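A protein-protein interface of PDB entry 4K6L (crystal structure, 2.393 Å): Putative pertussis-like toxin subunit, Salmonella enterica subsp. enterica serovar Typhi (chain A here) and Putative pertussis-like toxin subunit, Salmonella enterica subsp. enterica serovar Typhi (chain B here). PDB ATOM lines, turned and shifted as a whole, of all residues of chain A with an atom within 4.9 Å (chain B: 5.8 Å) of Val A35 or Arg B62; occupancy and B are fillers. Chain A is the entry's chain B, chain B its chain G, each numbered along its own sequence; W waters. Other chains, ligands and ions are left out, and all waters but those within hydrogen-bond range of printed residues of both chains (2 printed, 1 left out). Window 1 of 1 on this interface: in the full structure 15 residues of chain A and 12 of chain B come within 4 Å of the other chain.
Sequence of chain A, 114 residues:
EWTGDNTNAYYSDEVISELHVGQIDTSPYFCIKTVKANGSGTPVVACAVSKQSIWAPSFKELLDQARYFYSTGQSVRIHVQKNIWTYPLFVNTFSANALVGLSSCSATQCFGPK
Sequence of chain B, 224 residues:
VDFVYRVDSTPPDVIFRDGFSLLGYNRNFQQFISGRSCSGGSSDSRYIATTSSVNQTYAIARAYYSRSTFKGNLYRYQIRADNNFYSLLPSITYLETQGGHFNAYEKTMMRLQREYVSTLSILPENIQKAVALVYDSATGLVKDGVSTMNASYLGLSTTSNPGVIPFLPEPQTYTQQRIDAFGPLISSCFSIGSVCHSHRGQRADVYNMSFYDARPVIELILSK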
ATOM      1  N   ASP A  13     -15.650  33.636 -14.339  1.00  0.00           N
ATOM      2  CA  ASP A  13     -14.776  32.479 -14.200  1.00  0.00           C
ATOM      3  C   ASP A  13     -15.409  31.170 -14.663  1.00  0.00           C
ATOM      4  O   ASP A  13     -15.264  30.126 -14.009  1.00  0.00           O
ATOM      5  CB  ASP A  13     -14.328  32.365 -12.750  1.00  0.00           C
ATOM      6  CG  ASP A  13     -13.615  33.603 -12.277  1.00  0.00           C
ATOM      7  OD1 ASP A  13     -12.891  34.214 -13.088  1.00  0.00           O
ATOM      8  OD2 ASP A  13     -13.822  33.995 -11.111  1.00  0.00           O
ATOM      9  N   GLU A  14     -16.076  31.228 -15.810  1.00  0.00           N
ATOM     10  CA  GLU A  14     -16.728  30.058 -16.367  1.00  0.00           C
ATOM     11  C   GLU A  14     -15.911  29.518 -17.529  1.00  0.00           C
ATOM     12  O   GLU A  14     -15.103  30.229 -18.132  1.00  0.00           O
ATOM     13  CB  GLU A  14     -18.142  30.404 -16.841  1.00  0.00           C
ATOM     14  CG  GLU A  14     -19.081  30.959 -15.769  1.00  0.00           C
ATOM     15  CD  GLU A  14     -19.958  29.894 -15.128  1.00  0.00           C
ATOM     16  OE1 GLU A  14     -20.160  28.829 -15.745  1.00  0.00           O
ATOM     17  OE2 GLU A  14     -20.462  30.129 -14.010  1.00  0.00           O
ATOM     18  N   VAL A  15     -16.139  28.251 -17.844  1.00  0.00           N
ATOM     19  CA  VAL A  15     -15.506  27.606 -18.977  1.00  0.00           C
ATOM     20  C   VAL A  15     -16.616  27.175 -19.906  1.00  0.00           C
ATOM     21  O   VAL A  15     -17.573  26.546 -19.456  1.00  0.00           O
ATOM     22  CB  VAL A  15     -14.701  26.353 -18.537  1.00  0.00           C
ATOM     23  CG1 VAL A  15     -14.245  25.540 -19.745  1.00  0.00           C
ATOM     24  CG2 VAL A  15     -13.527  26.738 -17.653  1.00  0.00           C
ATOM     25  N   SER A  17     -18.139  24.750 -21.931  1.00  0.00           N
ATOM     26  CA  SER A  17     -17.869  23.316 -21.900  1.00  0.00           C
ATOM     27  C   SER A  17     -18.546  22.505 -23.002  1.00  0.00           C
ATOM     28  O   SER A  17     -18.060  21.433 -23.381  1.00  0.00           O
ATOM     29  CB  SER A  17     -18.253  22.747 -20.534  1.00  0.00           C
ATOM     30  OG  SER A  17     -19.623  22.985 -20.257  1.00  0.00           O
ATOM     31  N   LYS A  33     -22.906  25.691 -23.183  1.00  0.00           N
ATOM     32  CA  LYS A  33     -23.067  25.292 -21.797  1.00  0.00           C
ATOM     33  C   LYS A  33     -21.787  25.688 -21.102  1.00  0.00           C
ATOM     34  O   LYS A  33     -20.696  25.421 -21.610  1.00  0.00           O
ATOM     35  CB  LYS A  33     -23.305  23.789 -21.684  1.00  0.00           C
ATOM     36  CG  LYS A  33     -23.505  23.303 -20.257  1.00  0.00           C
ATOM     37  CD  LYS A  33     -23.893  21.829 -20.208  1.00  0.00           C
ATOM     38  CE  LYS A  33     -24.138  21.380 -18.773  1.00  0.00           C
ATOM     39  NZ  LYS A  33     -24.607  19.970 -18.669  1.00  0.00           N
ATOM     40  N   THR A  34     -21.908  26.389 -19.981  1.00  0.00           N
ATOM     41  CA  THR A  34     -20.724  26.826 -19.257  1.00  0.00           C
ATOM     42  C   THR A  34     -20.750  26.318 -17.832  1.00  0.00           C
ATOM     43  O   THR A  34     -21.819  26.179 -17.242  1.00  0.00           O
ATOM     44  CB  THR A  34     -20.585  28.375 -19.259  1.00  0.00           C
ATOM     45  OG1 THR A  34     -21.514  28.953 -18.333  1.00  0.00           O
ATOM     46  CG2 THR A  34     -20.848  28.939 -20.651  1.00  0.00           C
ATOM     47  N   VAL A  35     -19.572  26.039 -17.283  1.00  0.00           N
ATOM     48  CA  VAL A  35     -19.463  25.607 -15.894  1.00  0.00           C
ATOM     49  C   VAL A  35     -18.392  26.424 -15.176  1.00  0.00           C
ATOM     50  O   VAL A  35     -17.447  26.898 -15.806  1.00  0.00           O
ATOM     51  CB  VAL A  35     -19.105  24.110 -15.799  1.00  0.00           C
ATOM     52  CG1 VAL A  35     -20.222  23.259 -16.360  1.00  0.00           C
ATOM     53  CG2 VAL A  35     -17.812  23.820 -16.536  1.00  0.00           C
ATOM     54  N   LYS A  36     -18.539  26.596 -13.862  1.00  0.00           N
ATOM     55  CA  LYS A  36     -17.510  27.273 -13.087  1.00  0.00           C
ATOM     56  C   LYS A  36     -16.197  26.523 -13.219  1.00  0.00           C
ATOM     57  O   LYS A  36     -16.162  25.296 -13.117  1.00  0.00           O
ATOM     58  CB  LYS A  36     -17.904  27.355 -11.611  1.00  0.00           C
ATOM     59  CG  LYS A  36     -18.966  28.381 -11.296  1.00  0.00           C
ATOM     60  CD  LYS A  36     -18.387  29.788 -11.416  1.00  0.00           C
ATOM     61  CE  LYS A  36     -19.377  30.845 -10.973  1.00  0.00           C
ATOM     62  NZ  LYS A  36     -18.800  32.207 -11.064  1.00  0.00           N
ATOM     63  N   ALA A  37     -15.116  27.262 -13.437  1.00  0.00           N
ATOM     64  CA  ALA A  37     -13.811  26.643 -13.601  1.00  0.00           C
ATOM     65  C   ALA A  37     -13.372  25.919 -12.333  1.00  0.00           C
ATOM     66  O   ALA A  37     -12.727  24.877 -12.409  1.00  0.00           O
ATOM     67  CB  ALA A  37     -12.773  27.679 -14.016  1.00  0.00           C
ATOM     68  N   PRO A  43     -24.160  24.477 -13.861  1.00  0.00           N
ATOM     69  CA  PRO A  43     -23.896  24.946 -15.227  1.00  0.00           C
ATOM     70  C   PRO A  43     -24.915  25.962 -15.745  1.00  0.00           C
ATOM     71  O   PRO A  43     -26.094  25.920 -15.394  1.00  0.00           O
ATOM     72  CB  PRO A  43     -23.988  23.662 -16.050  1.00  0.00           C
ATOM     73  CG  PRO A  43     -23.559  22.604 -15.106  1.00  0.00           C
ATOM     74  CD  PRO A  43     -24.077  23.009 -13.764  1.00  0.00           C
ATOM     75  N   THR B  57      -5.430  21.737 -14.566  1.00  0.00           N
ATOM     76  CA  THR B  57      -5.490  20.351 -14.109  1.00  0.00           C
ATOM     77  C   THR B  57      -6.931  19.876 -14.125  1.00  0.00           C
ATOM     78  O   THR B  57      -7.201  18.705 -14.376  1.00  0.00           O
ATOM     79  CB  THR B  57      -4.876  20.139 -12.696  1.00  0.00           C
ATOM     80  OG1 THR B  57      -5.739  20.688 -11.691  1.00  0.00           O
ATOM     81  CG2 THR B  57      -3.493  20.770 -12.600  1.00  0.00           C
ATOM     82  N   TYR B  58      -7.862  20.784 -13.857  1.00  0.00           N
ATOM     83  CA  TYR B  58      -9.277  20.457 -13.999  1.00  0.00           C
ATOM     84  C   TYR B  58      -9.604  20.171 -15.465  1.00  0.00           C
ATOM     85  O   TYR B  58     -10.400  19.282 -15.773  1.00  0.00           O
ATOM     86  CB  TYR B  58     -10.165  21.584 -13.464  1.00  0.00           C
ATOM     87  CG  TYR B  58     -10.218  21.663 -11.953  1.00  0.00           C
ATOM     88  CD1 TYR B  58      -9.825  20.589 -11.167  1.00  0.00           C
ATOM     89  CD2 TYR B  58     -10.660  22.812 -11.313  1.00  0.00           C
ATOM     90  CE1 TYR B  58      -9.871  20.652  -9.788  1.00  0.00           C
ATOM     91  CE2 TYR B  58     -10.707  22.886  -9.929  1.00  0.00           C
ATOM     92  CZ  TYR B  58     -10.312  21.802  -9.174  1.00  0.00           C
ATOM     93  OH  TYR B  58     -10.361  21.866  -7.799  1.00  0.00           O
ATOM     94  N   ALA B  59      -8.971  20.913 -16.367  1.00  0.00           N
ATOM     95  CA  ALA B  59      -9.242  20.761 -17.794  1.00  0.00           C
ATOM     96  C   ALA B  59      -8.687  19.444 -18.319  1.00  0.00           C
ATOM     97  O   ALA B  59      -9.312  18.789 -19.149  1.00  0.00           O
ATOM     98  CB  ALA B  59      -8.679  21.938 -18.584  1.00  0.00           C
ATOM     99  N   ILE B  60      -7.512  19.067 -17.824  1.00  0.00           N
ATOM    100  CA  ILE B  60      -6.884  17.797 -18.172  1.00  0.00           C
ATOM    101  C   ILE B  60      -7.767  16.639 -17.726  1.00  0.00           C
ATOM    102  O   ILE B  60      -8.029  15.713 -18.494  1.00  0.00           O
ATOM    103  CB  ILE B  60      -5.488  17.662 -17.512  1.00  0.00           C
ATOM    104  CG1 ILE B  60      -4.518  18.701 -18.082  1.00  0.00           C
ATOM    105  CG2 ILE B  60      -4.917  16.272 -17.716  1.00  0.00           C
ATOM    106  CD1 ILE B  60      -3.204  18.789 -17.328  1.00  0.00           C
ATOM    107  N   ALA B  61      -8.236  16.710 -16.483  1.00  0.00           N
ATOM    108  CA  ALA B  61      -9.116  15.686 -15.926  1.00  0.00           C
ATOM    109  C   ALA B  61     -10.430  15.613 -16.687  1.00  0.00           C
ATOM    110  O   ALA B  61     -10.902  14.523 -17.017  1.00  0.00           O
ATOM    111  CB  ALA B  61      -9.367  15.939 -14.445  1.00  0.00           C
ATOM    112  N   ARG B  62     -11.012  16.776 -16.968  1.00  0.00           N
ATOM    113  CA  ARG B  62     -12.245  16.847 -17.751  1.00  0.00           C
ATOM    114  C   ARG B  62     -12.076  16.238 -19.140  1.00  0.00           C
ATOM    115  O   ARG B  62     -13.009  15.650 -19.680  1.00  0.00           O
ATOM    116  CB  ARG B  62     -12.762  18.286 -17.856  1.00  0.00           C
ATOM    117  CG  ARG B  62     -13.980  18.439 -18.770  1.00  0.00           C
ATOM    118  CD  ARG B  62     -14.528  19.854 -18.773  1.00  0.00           C
ATOM    119  NE  ARG B  62     -15.036  20.219 -17.459  1.00  0.00           N
ATOM    120  CZ  ARG B  62     -14.487  21.131 -16.665  1.00  0.00           C
ATOM    121  NH1 ARG B  62     -13.421  21.812 -17.061  1.00  0.00           N
ATOM    122  NH2 ARG B  62     -15.021  21.375 -15.478  1.00  0.00           N
ATOM    123  N   ALA B  63     -10.885  16.352 -19.715  1.00  0.00           N
ATOM    124  CA  ALA B  63     -10.678  15.830 -21.064  1.00  0.00           C
ATOM    125  C   ALA B  63     -10.620  14.306 -21.067  1.00  0.00           C
ATOM    126  O   ALA B  63     -10.888  13.676 -22.088  1.00  0.00           O
ATOM    127  CB  ALA B  63      -9.427  16.432 -21.706  1.00  0.00           C
ATOM    128  N   TYR B  64     -10.262  13.719 -19.924  1.00  0.00           N
ATOM    129  CA  TYR B  64     -10.294  12.262 -19.757  1.00  0.00           C
ATOM    130  C   TYR B  64     -11.673  11.800 -19.307  1.00  0.00           C
ATOM    131  O   TYR B  64     -12.240  10.864 -19.870  1.00  0.00           O
ATOM    132  CB  TYR B  64      -9.262  11.795 -18.728  1.00  0.00           C
ATOM    133  CG  TYR B  64      -7.855  11.691 -19.245  1.00  0.00           C
ATOM    134  CD1 TYR B  64      -7.394  10.522 -19.839  1.00  0.00           C
ATOM    135  CD2 TYR B  64      -6.980  12.753 -19.133  1.00  0.00           C
ATOM    136  CE1 TYR B  64      -6.095  10.424 -20.316  1.00  0.00           C
ATOM    137  CE2 TYR B  64      -5.686  12.668 -19.601  1.00  0.00           C
ATOM    138  CZ  TYR B  64      -5.248  11.510 -20.195  1.00  0.00           C
ATOM    139  OH  TYR B  64      -3.955  11.443 -20.659  1.00  0.00           O
ATOM    140  N   TYR B  65     -12.204  12.457 -18.281  1.00  0.00           N
ATOM    141  CA  TYR B  65     -13.485  12.060 -17.698  1.00  0.00           C
ATOM    142  C   TYR B  65     -14.653  12.194 -18.674  1.00  0.00           C
ATOM    143  O   TYR B  65     -15.636  11.464 -18.572  1.00  0.00           O
ATOM    144  CB  TYR B  65     -13.772  12.856 -16.420  1.00  0.00           C
ATOM    145  CG  TYR B  65     -13.042  12.366 -15.180  1.00  0.00           C
ATOM    146  CD1 TYR B  65     -13.066  11.022 -14.811  1.00  0.00           C
ATOM    147  CD2 TYR B  65     -12.336  13.253 -14.372  1.00  0.00           C
ATOM    148  CE1 TYR B  65     -12.406  10.579 -13.670  1.00  0.00           C
ATOM    149  CE2 TYR B  65     -11.673  12.820 -13.236  1.00  0.00           C
ATOM    150  CZ  TYR B  65     -11.713  11.483 -12.890  1.00  0.00           C
ATOM    151  OH  TYR B  65     -11.052  11.059 -11.767  1.00  0.00           O
ATOM    152  N   SER B  66     -14.542  13.117 -19.627  1.00  0.00           N
ATOM    153  CA  SER B  66     -15.623  13.348 -20.589  1.00  0.00           C
ATOM    154  C   SER B  66     -15.686  12.275 -21.668  1.00  0.00           C
ATOM    155  O   SER B  66     -16.615  12.255 -22.468  1.00  0.00           O
ATOM    156  CB  SER B  66     -15.502  14.729 -21.237  1.00  0.00           C
ATOM    157  OG  SER B  66     -14.254  14.879 -21.893  1.00  0.00           O
ATOM    158  N   ARG B  67     -14.694  11.391 -21.695  1.00  0.00           N
ATOM    159  CA  ARG B  67     -14.702  10.274 -22.635  1.00  0.00           C
ATOM    160  C   ARG B  67     -15.362   9.051 -21.999  1.00  0.00           C
ATOM    161  O   ARG B  67     -15.070   8.697 -20.857  1.00  0.00           O
ATOM    162  CB  ARG B  67     -13.283   9.941 -23.092  1.00  0.00           C
ATOM    163  CG  ARG B  67     -12.456  11.157 -23.441  1.00  0.00           C
ATOM    164  CD  ARG B  67     -11.023  10.789 -23.771  1.00  0.00           C
ATOM    165  NE  ARG B  67     -10.896  10.277 -25.131  1.00  0.00           N
ATOM    166  CZ  ARG B  67     -10.800  11.044 -26.214  1.00  0.00           C
ATOM    167  NH1 ARG B  67     -10.821  12.365 -26.103  1.00  0.00           N
ATOM    168  NH2 ARG B  67     -10.688  10.487 -27.412  1.00  0.00           N
ATOM    169  N   LEU B  74      -8.569   9.959 -11.312  1.00  0.00           N
ATOM    170  CA  LEU B  74      -7.482  10.894 -11.564  1.00  0.00           C
ATOM    171  C   LEU B  74      -7.111  11.674 -10.317  1.00  0.00           C
ATOM    172  O   LEU B  74      -7.972  11.998  -9.499  1.00  0.00           O
ATOM    173  CB  LEU B  74      -7.869  11.862 -12.689  1.00  0.00           C
ATOM    174  CG  LEU B  74      -8.164  11.188 -14.028  1.00  0.00           C
ATOM    175  CD1 LEU B  74      -8.468  12.223 -15.098  1.00  0.00           C
ATOM    176  CD2 LEU B  74      -6.992  10.322 -14.437  1.00  0.00           C
ATOM    177  N   TYR B 135     -15.343  13.796 -10.828  1.00  0.00           N
ATOM    178  CA  TYR B 135     -16.137  14.244 -11.962  1.00  0.00           C
ATOM    179  C   TYR B 135     -17.620  13.947 -11.799  1.00  0.00           C
ATOM    180  O   TYR B 135     -18.013  12.800 -11.611  1.00  0.00           O
ATOM    181  CB  TYR B 135     -15.623  13.574 -13.231  1.00  0.00           C
ATOM    182  CG  TYR B 135     -16.217  14.105 -14.514  1.00  0.00           C
ATOM    183  CD1 TYR B 135     -15.849  15.345 -15.007  1.00  0.00           C
ATOM    184  CD2 TYR B 135     -17.111  13.344 -15.254  1.00  0.00           C
ATOM    185  CE1 TYR B 135     -16.378  15.830 -16.190  1.00  0.00           C
ATOM    186  CE2 TYR B 135     -17.642  13.816 -16.436  1.00  0.00           C
ATOM    187  CZ  TYR B 135     -17.273  15.060 -16.901  1.00  0.00           C
ATOM    188  OH  TYR B 135     -17.800  15.534 -18.083  1.00  0.00           O
ATOM    189  N   THR B 139     -23.029  17.231 -14.842  1.00  0.00           N
ATOM    190  CA  THR B 139     -22.803  18.661 -14.979  1.00  0.00           C
ATOM    191  C   THR B 139     -21.515  18.983 -15.721  1.00  0.00           C
ATOM    192  O   THR B 139     -21.382  20.058 -16.298  1.00  0.00           O
ATOM    193  CB  THR B 139     -22.763  19.346 -13.600  1.00  0.00           C
ATOM    194  OG1 THR B 139     -21.768  18.721 -12.785  1.00  0.00           O
ATOM    195  CG2 THR B 139     -24.103  19.226 -12.912  1.00  0.00           C
ATOM    196  N   GLY B 140     -20.571  18.046 -15.702  1.00  0.00           N
ATOM    197  CA  GLY B 140     -19.250  18.278 -16.257  1.00  0.00           C
ATOM    198  C   GLY B 140     -18.335  18.969 -15.262  1.00  0.00           C
ATOM    199  O   GLY B 140     -17.186  19.277 -15.567  1.00  0.00           O
ATOM    200  N   LEU B 141     -18.851  19.222 -14.065  1.00  0.00           N
ATOM    201  CA  LEU B 141     -18.068  19.869 -13.022  1.00  0.00           C
ATOM    202  C   LEU B 141     -16.971  18.948 -12.505  1.00  0.00           C
ATOM    203  O   LEU B 141     -17.187  17.751 -12.315  1.00  0.00           O
ATOM    204  CB  LEU B 141     -18.969  20.309 -11.864  1.00  0.00           C
ATOM    205  CG  LEU B 141     -19.898  21.485 -12.175  1.00  0.00           C
ATOM    206  CD1 LEU B 141     -20.871  21.743 -11.033  1.00  0.00           C
ATOM    207  CD2 LEU B 141     -19.086  22.728 -12.480  1.00  0.00           C
ATOM    208  N   VAL B 142     -15.792  19.517 -12.289  1.00  0.00           N
ATOM    209  CA  VAL B 142     -14.694  18.803 -11.661  1.00  0.00           C
ATOM    210  C   VAL B 142     -14.416  19.444 -10.303  1.00  0.00           C
ATOM    211  O   VAL B 142     -14.257  20.655 -10.212  1.00  0.00           O
ATOM    212  CB  VAL B 142     -13.430  18.832 -12.537  1.00  0.00           C
ATOM    213  CG1 VAL B 142     -12.266  18.169 -11.813  1.00  0.00           C
ATOM    214  CG2 VAL B 142     -13.694  18.131 -13.859  1.00  0.00           C
HETATM  215  O   HOH W   1     -12.650  23.765 -15.260  1.00  0.00           O
HETATM  216  O   HOH W   2     -14.741  22.514 -12.873  1.00  0.00           O
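Val A35 touches three residues of chain B. Printed residues of chain B within 4 Å of Lys A36: Leu B141 (3.9 Å). Of the printed residues of chain B, Ala A37 touches Tyr B58 (3.1 Å). Of the printed residues of chain A, Tyr B58 touches Ala A37 (3.1 Å). Arg B62 touches just one residue of chain A: Val A35. Tyr B65 touches none of the printed residues of chain A. The nearest printed residue of chain A that does not touch Thr B139 is Ser A17 (5.2 Å).
The backbone NH of Ala A37 lies within hydrogen-bond range of the backbone carbonyl oxygen of Asp A13 (2.9 Å). The backbone NH (N) of Ser A17 is in hydrogen-bond range of the backbone carbonyl oxygen (O) of Lys A33 (2.7 Å). N of Val A15 lies within hydrogen-bond range of O of Val A35 (2.8 Å). The side-chain hydroxyl (OG1) of Thr B139 sits close to the backbone NH (N) of Leu B141 (3.2 Å). NZ of Lys A36 lies within salt-bridge range of OE2 of Glu A14, 3.97 Å away. The side-chain hydroxyl (OG) of Ser B66 sits at hydrogen-bond distance from the backbone carbonyl oxygen (O) of Arg B62.
Of the 17 printed residues of chain B, 4 touch a printed residue of chain A. Hydrophobic or aromatic side chains of chain B that line the printed part of chain A: Tyr B58 and Leu B141. Among the printed residues, 7 pairs touch across the chains. Among the printed residues, no Asp or Glu carboxylate lies within 4 Å of a Lys or Arg side-chain nitrogen of the other chain.
Water W1 bridges the guanidinium group of Arg B62 (2.8 Å) and the backbone carbonyl oxygen of Ala A37 (3.1 Å). Water W2 lies within hydrogen-bond range of NH2 of Arg B62 (2.9 Å), O of Lys A36 (3.1 Å), O of Ala A37 (3.1 Å) and N of Val B142 (3.2 Å).
Lys A33 touches Thr B139. Arg B62 touches Val A35 (NH2 to CG2, 3.9 Å). Thr B139 touches Val A35. Val A35 touches Leu B141 (CB to CD2, 3.6 Å). Leu B141 touches Lys A36 (CD2 to O, 3.9 Å). Ala A37 touches Tyr B58. O of Thr B139 touches CG of Pro A43, 3.6 Å away.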
